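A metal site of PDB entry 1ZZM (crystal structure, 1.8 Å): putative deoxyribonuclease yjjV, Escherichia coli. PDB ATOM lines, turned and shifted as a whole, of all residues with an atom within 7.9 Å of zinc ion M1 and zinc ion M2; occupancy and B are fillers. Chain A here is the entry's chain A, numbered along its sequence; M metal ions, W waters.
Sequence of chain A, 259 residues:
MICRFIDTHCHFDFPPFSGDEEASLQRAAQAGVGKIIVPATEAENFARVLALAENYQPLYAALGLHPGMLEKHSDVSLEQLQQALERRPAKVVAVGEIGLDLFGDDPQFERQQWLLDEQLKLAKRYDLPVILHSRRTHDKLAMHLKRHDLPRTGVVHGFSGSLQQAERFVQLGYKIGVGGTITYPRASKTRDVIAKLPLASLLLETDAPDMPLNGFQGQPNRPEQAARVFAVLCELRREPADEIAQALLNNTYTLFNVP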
ATOM      1  N   HIS A   9      -5.478 -29.080   2.407  1.00  0.00           N
ATOM      2  CA  HIS A   9      -6.887 -28.678   2.352  1.00  0.00           C
ATOM      3  C   HIS A   9      -7.636 -29.271   3.557  1.00  0.00           C
ATOM      4  O   HIS A   9      -8.072 -30.411   3.520  1.00  0.00           O
ATOM      5  CB  HIS A   9      -7.502 -29.228   1.045  1.00  0.00           C
ATOM      6  CG  HIS A   9      -8.826 -28.614   0.693  1.00  0.00           C
ATOM      7  ND1 HIS A   9      -8.964 -27.664  -0.292  1.00  0.00           N
ATOM      8  CD2 HIS A   9     -10.060 -28.838   1.187  1.00  0.00           C
ATOM      9  CE1 HIS A   9     -10.249 -27.331  -0.389  1.00  0.00           C
ATOM     10  NE2 HIS A   9     -10.924 -28.027   0.505  1.00  0.00           N
ATOM     11  N   CYS A  10      -7.736 -28.505   4.627  1.00  0.00           N
ATOM     12  CA  CYS A  10      -8.455 -28.971   5.792  1.00  0.00           C
ATOM     13  C   CYS A  10      -9.276 -27.816   6.349  1.00  0.00           C
ATOM     14  O   CYS A  10      -8.742 -26.735   6.626  1.00  0.00           O
ATOM     15  CB  CYS A  10      -7.465 -29.472   6.867  1.00  0.00           C
ATOM     16  SG  CYS A  10      -8.322 -29.997   8.424  1.00  0.00           S
ATOM     17  N   HIS A  11     -10.591 -28.034   6.510  1.00  0.00           N
ATOM     18  CA  HIS A  11     -11.484 -27.004   7.029  1.00  0.00           C
ATOM     19  C   HIS A  11     -11.378 -27.055   8.549  1.00  0.00           C
ATOM     20  O   HIS A  11     -12.320 -27.427   9.257  1.00  0.00           O
ATOM     21  CB  HIS A  11     -12.911 -27.284   6.543  1.00  0.00           C
ATOM     22  CG  HIS A  11     -13.076 -27.074   5.074  1.00  0.00           C
ATOM     23  ND1 HIS A  11     -13.188 -25.825   4.515  1.00  0.00           N
ATOM     24  CD2 HIS A  11     -13.028 -27.947   4.030  1.00  0.00           C
ATOM     25  CE1 HIS A  11     -13.187 -25.918   3.200  1.00  0.00           C
ATOM     26  NE2 HIS A  11     -13.084 -27.201   2.876  1.00  0.00           N
ATOM     27  N   PRO A  39      -8.652 -23.433   3.932  1.00  0.00           N
ATOM     28  CA  PRO A  39      -9.333 -22.539   2.992  1.00  0.00           C
ATOM     29  C   PRO A  39     -10.676 -22.076   3.550  1.00  0.00           C
ATOM     30  O   PRO A  39     -11.436 -22.894   4.104  1.00  0.00           O
ATOM     31  CB  PRO A  39      -9.463 -23.388   1.746  1.00  0.00           C
ATOM     32  CG  PRO A  39      -9.586 -24.781   2.260  1.00  0.00           C
ATOM     33  CD  PRO A  39      -8.836 -24.851   3.570  1.00  0.00           C
ATOM     34  N   ALA A  40     -10.985 -20.789   3.435  1.00  0.00           N
ATOM     35  CA  ALA A  40     -12.269 -20.307   3.975  1.00  0.00           C
ATOM     36  C   ALA A  40     -13.402 -20.697   3.043  1.00  0.00           C
ATOM     37  O   ALA A  40     -13.166 -21.114   1.897  1.00  0.00           O
ATOM     38  CB  ALA A  40     -12.252 -18.826   4.151  1.00  0.00           C
ATOM     39  N   THR A  41     -14.641 -20.554   3.535  1.00  0.00           N
ATOM     40  CA  THR A  41     -15.848 -20.885   2.767  1.00  0.00           C
ATOM     41  C   THR A  41     -16.743 -19.694   2.505  1.00  0.00           C
ATOM     42  O   THR A  41     -17.557 -19.699   1.569  1.00  0.00           O
ATOM     43  CB  THR A  41     -16.696 -21.923   3.515  1.00  0.00           C
ATOM     44  OG1 THR A  41     -16.984 -21.429   4.837  1.00  0.00           O
ATOM     45  CG2 THR A  41     -15.911 -23.290   3.613  1.00  0.00           C
ATOM     46  N   HIS A  66     -16.782 -20.136  -1.202  1.00  0.00           N
ATOM     47  CA  HIS A  66     -17.105 -21.497  -1.645  1.00  0.00           C
ATOM     48  C   HIS A  66     -18.438 -21.586  -2.379  1.00  0.00           C
ATOM     49  O   HIS A  66     -19.438 -21.000  -1.950  1.00  0.00           O
ATOM     50  CB  HIS A  66     -17.086 -22.398  -0.385  1.00  0.00           C
ATOM     51  CG  HIS A  66     -16.978 -23.868  -0.674  1.00  0.00           C
ATOM     52  ND1 HIS A  66     -17.959 -24.562  -1.364  1.00  0.00           N
ATOM     53  CD2 HIS A  66     -16.084 -24.797  -0.258  1.00  0.00           C
ATOM     54  CE1 HIS A  66     -17.661 -25.854  -1.353  1.00  0.00           C
ATOM     55  NE2 HIS A  66     -16.536 -26.022  -0.682  1.00  0.00           N
ATOM     56  N   PRO A  67     -18.481 -22.320  -3.509  1.00  0.00           N
ATOM     57  CA  PRO A  67     -19.754 -22.427  -4.259  1.00  0.00           C
ATOM     58  C   PRO A  67     -20.871 -23.071  -3.441  1.00  0.00           C
ATOM     59  O   PRO A  67     -22.056 -22.788  -3.678  1.00  0.00           O
ATOM     60  CB  PRO A  67     -19.368 -23.245  -5.503  1.00  0.00           C
ATOM     61  CG  PRO A  67     -18.195 -24.092  -5.039  1.00  0.00           C
ATOM     62  CD  PRO A  67     -17.420 -23.109  -4.156  1.00  0.00           C
ATOM     63  N   GLU A  97     -10.903 -21.368  -1.368  1.00  0.00           N
ATOM     64  CA  GLU A  97     -11.894 -22.338  -1.643  1.00  0.00           C
ATOM     65  C   GLU A  97     -12.929 -21.627  -2.462  1.00  0.00           C
ATOM     66  O   GLU A  97     -13.861 -21.020  -1.956  1.00  0.00           O
ATOM     67  CB  GLU A  97     -12.470 -23.296  -0.619  1.00  0.00           C
ATOM     68  CG  GLU A  97     -12.858 -24.455  -1.597  1.00  0.00           C
ATOM     69  CD  GLU A  97     -13.153 -25.822  -1.006  1.00  0.00           C
ATOM     70  OE1 GLU A  97     -13.145 -26.013   0.226  1.00  0.00           O
ATOM     71  OE2 GLU A  97     -13.385 -26.728  -1.835  1.00  0.00           O
ATOM     72  N   ILE A  98     -12.661 -21.659  -3.763  1.00  0.00           N
ATOM     73  CA  ILE A  98     -13.566 -21.070  -4.756  1.00  0.00           C
ATOM     74  C   ILE A  98     -13.743 -22.205  -5.760  1.00  0.00           C
ATOM     75  O   ILE A  98     -13.018 -23.201  -5.698  1.00  0.00           O
ATOM     76  CB  ILE A  98     -12.960 -19.869  -5.463  1.00  0.00           C
ATOM     77  CG1 ILE A  98     -11.753 -20.298  -6.310  1.00  0.00           C
ATOM     78  CG2 ILE A  98     -12.544 -18.839  -4.433  1.00  0.00           C
ATOM     79  CD1 ILE A  98     -11.002 -19.123  -6.916  1.00  0.00           C
ATOM     80  N   LEU A 100     -16.728 -24.448  -8.518  1.00  0.00           N
ATOM     81  CA  LEU A 100     -18.050 -24.747  -9.017  1.00  0.00           C
ATOM     82  C   LEU A 100     -18.533 -26.082  -8.489  1.00  0.00           C
ATOM     83  O   LEU A 100     -17.738 -26.967  -8.157  1.00  0.00           O
ATOM     84  CB  LEU A 100     -18.022 -24.842 -10.542  1.00  0.00           C
ATOM     85  CG  LEU A 100     -17.352 -23.651 -11.246  1.00  0.00           C
ATOM     86  CD1 LEU A 100     -17.050 -24.085 -12.636  1.00  0.00           C
ATOM     87  CD2 LEU A 100     -18.244 -22.381 -11.203  1.00  0.00           C
ATOM     88  N   ASP A 101     -19.846 -26.261  -8.429  1.00  0.00           N
ATOM     89  CA  ASP A 101     -20.374 -27.514  -7.890  1.00  0.00           C
ATOM     90  C   ASP A 101     -21.780 -27.663  -8.470  1.00  0.00           C
ATOM     91  O   ASP A 101     -22.662 -26.860  -8.153  1.00  0.00           O
ATOM     92  CB  ASP A 101     -20.414 -27.380  -6.377  1.00  0.00           C
ATOM     93  CG  ASP A 101     -20.832 -28.656  -5.667  1.00  0.00           C
ATOM     94  OD1 ASP A 101     -21.699 -29.347  -6.206  1.00  0.00           O
ATOM     95  OD2 ASP A 101     -20.284 -28.961  -4.580  1.00  0.00           O
ATOM     96  N   ILE A 131      -7.257 -22.254  -4.727  1.00  0.00           N
ATOM     97  CA  ILE A 131      -7.600 -23.589  -4.236  1.00  0.00           C
ATOM     98  C   ILE A 131      -9.010 -23.762  -4.764  1.00  0.00           C
ATOM     99  O   ILE A 131      -9.946 -23.048  -4.383  1.00  0.00           O
ATOM    100  CB  ILE A 131      -7.573 -23.654  -2.686  1.00  0.00           C
ATOM    101  CG1 ILE A 131      -6.103 -23.698  -2.221  1.00  0.00           C
ATOM    102  CG2 ILE A 131      -8.337 -24.896  -2.183  1.00  0.00           C
ATOM    103  CD1 ILE A 131      -5.938 -23.746  -0.648  1.00  0.00           C
ATOM    104  N   LEU A 132      -9.148 -24.727  -5.653  1.00  0.00           N
ATOM    105  CA  LEU A 132     -10.388 -24.953  -6.345  1.00  0.00           C
ATOM    106  C   LEU A 132     -11.164 -26.201  -5.977  1.00  0.00           C
ATOM    107  O   LEU A 132     -10.601 -27.290  -5.787  1.00  0.00           O
ATOM    108  CB  LEU A 132     -10.105 -24.990  -7.852  1.00  0.00           C
ATOM    109  CG  LEU A 132      -9.479 -23.750  -8.479  1.00  0.00           C
ATOM    110  CD1 LEU A 132      -8.777 -24.153  -9.803  1.00  0.00           C
ATOM    111  CD2 LEU A 132     -10.562 -22.681  -8.706  1.00  0.00           C
ATOM    112  N   HIS A 133     -12.487 -26.004  -5.932  1.00  0.00           N
ATOM    113  CA  HIS A 133     -13.480 -27.033  -5.667  1.00  0.00           C
ATOM    114  C   HIS A 133     -14.155 -27.273  -7.009  1.00  0.00           C
ATOM    115  O   HIS A 133     -14.494 -26.319  -7.732  1.00  0.00           O
ATOM    116  CB  HIS A 133     -14.529 -26.505  -4.680  1.00  0.00           C
ATOM    117  CG  HIS A 133     -15.636 -27.471  -4.374  1.00  0.00           C
ATOM    118  ND1 HIS A 133     -15.586 -28.370  -3.337  1.00  0.00           N
ATOM    119  CD2 HIS A 133     -16.862 -27.629  -4.931  1.00  0.00           C
ATOM    120  CE1 HIS A 133     -16.720 -29.035  -3.253  1.00  0.00           C
ATOM    121  NE2 HIS A 133     -17.514 -28.612  -4.218  1.00  0.00           N
ATOM    122  N   SER A 134     -14.357 -28.541  -7.367  1.00  0.00           N
ATOM    123  CA  SER A 134     -15.006 -28.872  -8.627  1.00  0.00           C
ATOM    124  C   SER A 134     -15.751 -30.174  -8.440  1.00  0.00           C
ATOM    125  O   SER A 134     -15.146 -31.206  -8.127  1.00  0.00           O
ATOM    126  CB  SER A 134     -13.987 -29.021  -9.756  1.00  0.00           C
ATOM    127  OG  SER A 134     -14.660 -29.156 -11.028  1.00  0.00           O
ATOM    128  N   ARG A 135     -17.059 -30.138  -8.609  1.00  0.00           N
ATOM    129  CA  ARG A 135     -17.812 -31.355  -8.441  1.00  0.00           C
ATOM    130  C   ARG A 135     -18.770 -31.419  -9.631  1.00  0.00           C
ATOM    131  O   ARG A 135     -19.755 -30.650  -9.703  1.00  0.00           O
ATOM    132  CB  ARG A 135     -18.570 -31.287  -7.126  1.00  0.00           C
ATOM    133  CG  ARG A 135     -19.510 -32.447  -6.911  1.00  0.00           C
ATOM    134  CD  ARG A 135     -20.541 -32.026  -5.889  1.00  0.00           C
ATOM    135  NE  ARG A 135     -20.671 -32.994  -4.825  1.00  0.00           N
ATOM    136  CZ  ARG A 135     -21.067 -32.667  -3.596  1.00  0.00           C
ATOM    137  NH1 ARG A 135     -21.346 -31.391  -3.324  1.00  0.00           N
ATOM    138  NH2 ARG A 135     -21.165 -33.605  -2.668  1.00  0.00           N
ATOM    139  N   HIS A 157      -8.589 -29.263  -5.926  1.00  0.00           N
ATOM    140  CA  HIS A 157      -8.573 -30.154  -4.756  1.00  0.00           C
ATOM    141  C   HIS A 157      -9.552 -31.332  -4.818  1.00  0.00           C
ATOM    142  O   HIS A 157     -10.506 -31.332  -5.601  1.00  0.00           O
ATOM    143  CB  HIS A 157      -8.828 -29.309  -3.502  1.00  0.00           C
ATOM    144  CG  HIS A 157     -10.183 -29.519  -2.893  1.00  0.00           C
ATOM    145  ND1 HIS A 157     -10.472 -30.590  -2.065  1.00  0.00           N
ATOM    146  CD2 HIS A 157     -11.344 -28.837  -3.052  1.00  0.00           C
ATOM    147  CE1 HIS A 157     -11.756 -30.550  -1.744  1.00  0.00           C
ATOM    148  NE2 HIS A 157     -12.308 -29.499  -2.321  1.00  0.00           N
ATOM    149  N   GLY A 158      -9.264 -32.349  -3.998  1.00  0.00           N
ATOM    150  CA  GLY A 158     -10.127 -33.519  -3.869  1.00  0.00           C
ATOM    151  C   GLY A 158     -10.590 -34.068  -5.193  1.00  0.00           C
ATOM    152  O   GLY A 158     -11.710 -34.482  -5.332  1.00  0.00           O
ATOM    153  N   GLU A 205      -3.931 -34.129   0.646  1.00  0.00           N
ATOM    154  CA  GLU A 205      -4.956 -33.393   1.413  1.00  0.00           C
ATOM    155  C   GLU A 205      -5.926 -34.369   2.031  1.00  0.00           C
ATOM    156  O   GLU A 205      -5.828 -35.577   1.779  1.00  0.00           O
ATOM    157  CB  GLU A 205      -5.787 -32.496   0.500  1.00  0.00           C
ATOM    158  CG  GLU A 205      -6.690 -33.324  -0.426  1.00  0.00           C
ATOM    159  CD  GLU A 205      -7.613 -32.483  -1.280  1.00  0.00           C
ATOM    160  OE1 GLU A 205      -7.113 -31.787  -2.184  1.00  0.00           O
ATOM    161  OE2 GLU A 205      -8.833 -32.537  -1.076  1.00  0.00           O
ATOM    162  N   THR A 206      -6.853 -33.839   2.833  1.00  0.00           N
ATOM    163  CA  THR A 206      -7.937 -34.655   3.405  1.00  0.00           C
ATOM    164  C   THR A 206      -9.350 -34.089   3.162  1.00  0.00           C
ATOM    165  O   THR A 206     -10.316 -34.851   3.066  1.00  0.00           O
ATOM    166  CB  THR A 206      -7.883 -34.813   4.951  1.00  0.00           C
ATOM    167  OG1 THR A 206      -7.949 -33.517   5.565  1.00  0.00           O
ATOM    168  CG2 THR A 206      -6.609 -35.588   5.403  1.00  0.00           C
ATOM    169  N   ASP A 207      -9.452 -32.764   3.070  1.00  0.00           N
ATOM    170  CA  ASP A 207     -10.724 -32.050   2.996  1.00  0.00           C
ATOM    171  C   ASP A 207     -11.475 -32.325   4.314  1.00  0.00           C
ATOM    172  O   ASP A 207     -12.706 -32.246   4.385  1.00  0.00           O
ATOM    173  CB  ASP A 207     -11.628 -32.456   1.789  1.00  0.00           C
ATOM    174  CG  ASP A 207     -12.777 -31.440   1.551  1.00  0.00           C
ATOM    175  OD1 ASP A 207     -12.687 -30.296   2.040  1.00  0.00           O
ATOM    176  OD2 ASP A 207     -13.766 -31.772   0.873  1.00  0.00           O
ATOM    177  N   ALA A 208     -10.747 -32.660   5.378  1.00  0.00           N
ATOM    178  CA  ALA A 208     -11.419 -32.921   6.666  1.00  0.00           C
ATOM    179  C   ALA A 208     -12.211 -31.682   7.090  1.00  0.00           C
ATOM    180  O   ALA A 208     -11.763 -30.550   6.912  1.00  0.00           O
ATOM    181  CB  ALA A 208     -10.386 -33.287   7.760  1.00  0.00           C
ATOM    182  N   PRO A 209     -13.341 -31.879   7.770  1.00  0.00           N
ATOM    183  CA  PRO A 209     -13.958 -33.132   8.196  1.00  0.00           C
ATOM    184  C   PRO A 209     -14.720 -33.922   7.155  1.00  0.00           C
ATOM    185  O   PRO A 209     -15.271 -34.968   7.462  1.00  0.00           O
ATOM    186  CB  PRO A 209     -14.846 -32.679   9.364  1.00  0.00           C
ATOM    187  CG  PRO A 209     -15.398 -31.428   8.811  1.00  0.00           C
ATOM    188  CD  PRO A 209     -14.167 -30.740   8.205  1.00  0.00           C
ATOM    189  N   ASP A 210     -14.787 -33.436   5.913  1.00  0.00           N
ATOM    190  CA  ASP A 210     -15.528 -34.209   4.906  1.00  0.00           C
ATOM    191  C   ASP A 210     -14.627 -35.251   4.239  1.00  0.00           C
ATOM    192  O   ASP A 210     -13.456 -35.394   4.623  1.00  0.00           O
ATOM    193  CB  ASP A 210     -16.118 -33.263   3.844  1.00  0.00           C
ATOM    194  CG  ASP A 210     -17.084 -32.235   4.452  1.00  0.00           C
ATOM    195  OD1 ASP A 210     -17.706 -32.520   5.512  1.00  0.00           O
ATOM    196  OD2 ASP A 210     -17.239 -31.140   3.860  1.00  0.00           O
ATOM    197  N   MET A 211     -15.174 -35.990   3.258  1.00  0.00           N
ATOM    198  CA  MET A 211     -14.438 -37.021   2.511  1.00  0.00           C
ATOM    199  C   MET A 211     -13.749 -38.082   3.401  1.00  0.00           C
ATOM    200  O   MET A 211     -12.546 -38.328   3.287  1.00  0.00           O
ATOM    201  CB  MET A 211     -13.435 -36.340   1.550  1.00  0.00           C
ATOM    202  CG  MET A 211     -14.123 -35.341   0.530  1.00  0.00           C
ATOM    203  SD  MET A 211     -13.071 -34.474  -0.776  1.00  0.00           S
ATOM    204  CE  MET A 211     -13.046 -35.713  -2.094  1.00  0.00           C
HETATM  205 ZN    ZN M   1     -12.946 -27.857   0.993  1.00  0.00          ZN
HETATM  206 ZN    ZN M   2     -14.189 -28.695  -1.883  1.00  0.00          ZN
HETATM  207  O   HOH W   1     -15.103 -30.911  -1.530  1.00  0.00           O
HETATM  208  O   HOH W   2     -14.656 -28.458   0.082  1.00  0.00           O
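Five residues have an atom within 4 Å of zinc ion M1: His 9, His 11, Glu 97, His 157 and Asp 207. The nearest printed residue that does not touch zinc ion M1 is His 66 (4.4 Å).
His 66 touches zinc ion M2 (NE2 to ZN, 3.8 Å).
A ring nitrogen (NE2) of His 133 lies within hydrogen-bond range of the side-chain carboxylate of Asp 101, 2.8 Å away. N of His 133 sits at hydrogen-bond distance from O of Ile 98. N of His 66 is in hydrogen-bond range of O of Glu 97, 3.1 Å away. N of Asp 207 is in hydrogen-bond range of O of His 9 (2.8 Å). The backbone carbonyl oxygen (O) of Pro 39 sits at hydrogen-bond distance from a ring nitrogen (ND1) of His 11. N of His 66 sits at hydrogen-bond distance from O of Thr 41 (2.9 Å). N of His 157 is in hydrogen-bond range of O of Leu 132. The backbone NH (N) of Leu 100 lies within hydrogen-bond range of the backbone carbonyl oxygen (O) of His 133 (3.0 Å).
NE2 of His 11 is bound to zinc ion M1, at 2.0 Å. OE1 of Glu 97 binds zinc ion M1 (2.0 Å). Water W2 is bound to zinc ion M1 (2.0 Å). NE2 of His 9 binds zinc ion M1 (2.1 Å). Zinc ion M1 has four donor atoms within binding distance. Slightly farther from zinc ion M1 lies the side-chain carboxylate (OD1) of Asp 207 (2.7 Å).
Zinc ion M2 is bound by water W2 (2.0 Å), ND1 of His 133 (2.0 Å), NE2 of His 157 (2.1 Å), OE2 of Glu 97 (2.1 Å) and water W1 (2.4 Å).
Water W2 bridges a ring nitrogen (NE2) of His 66 (3.2 Å) and the side-chain carboxylate of Asp 207 (3.3 Å).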
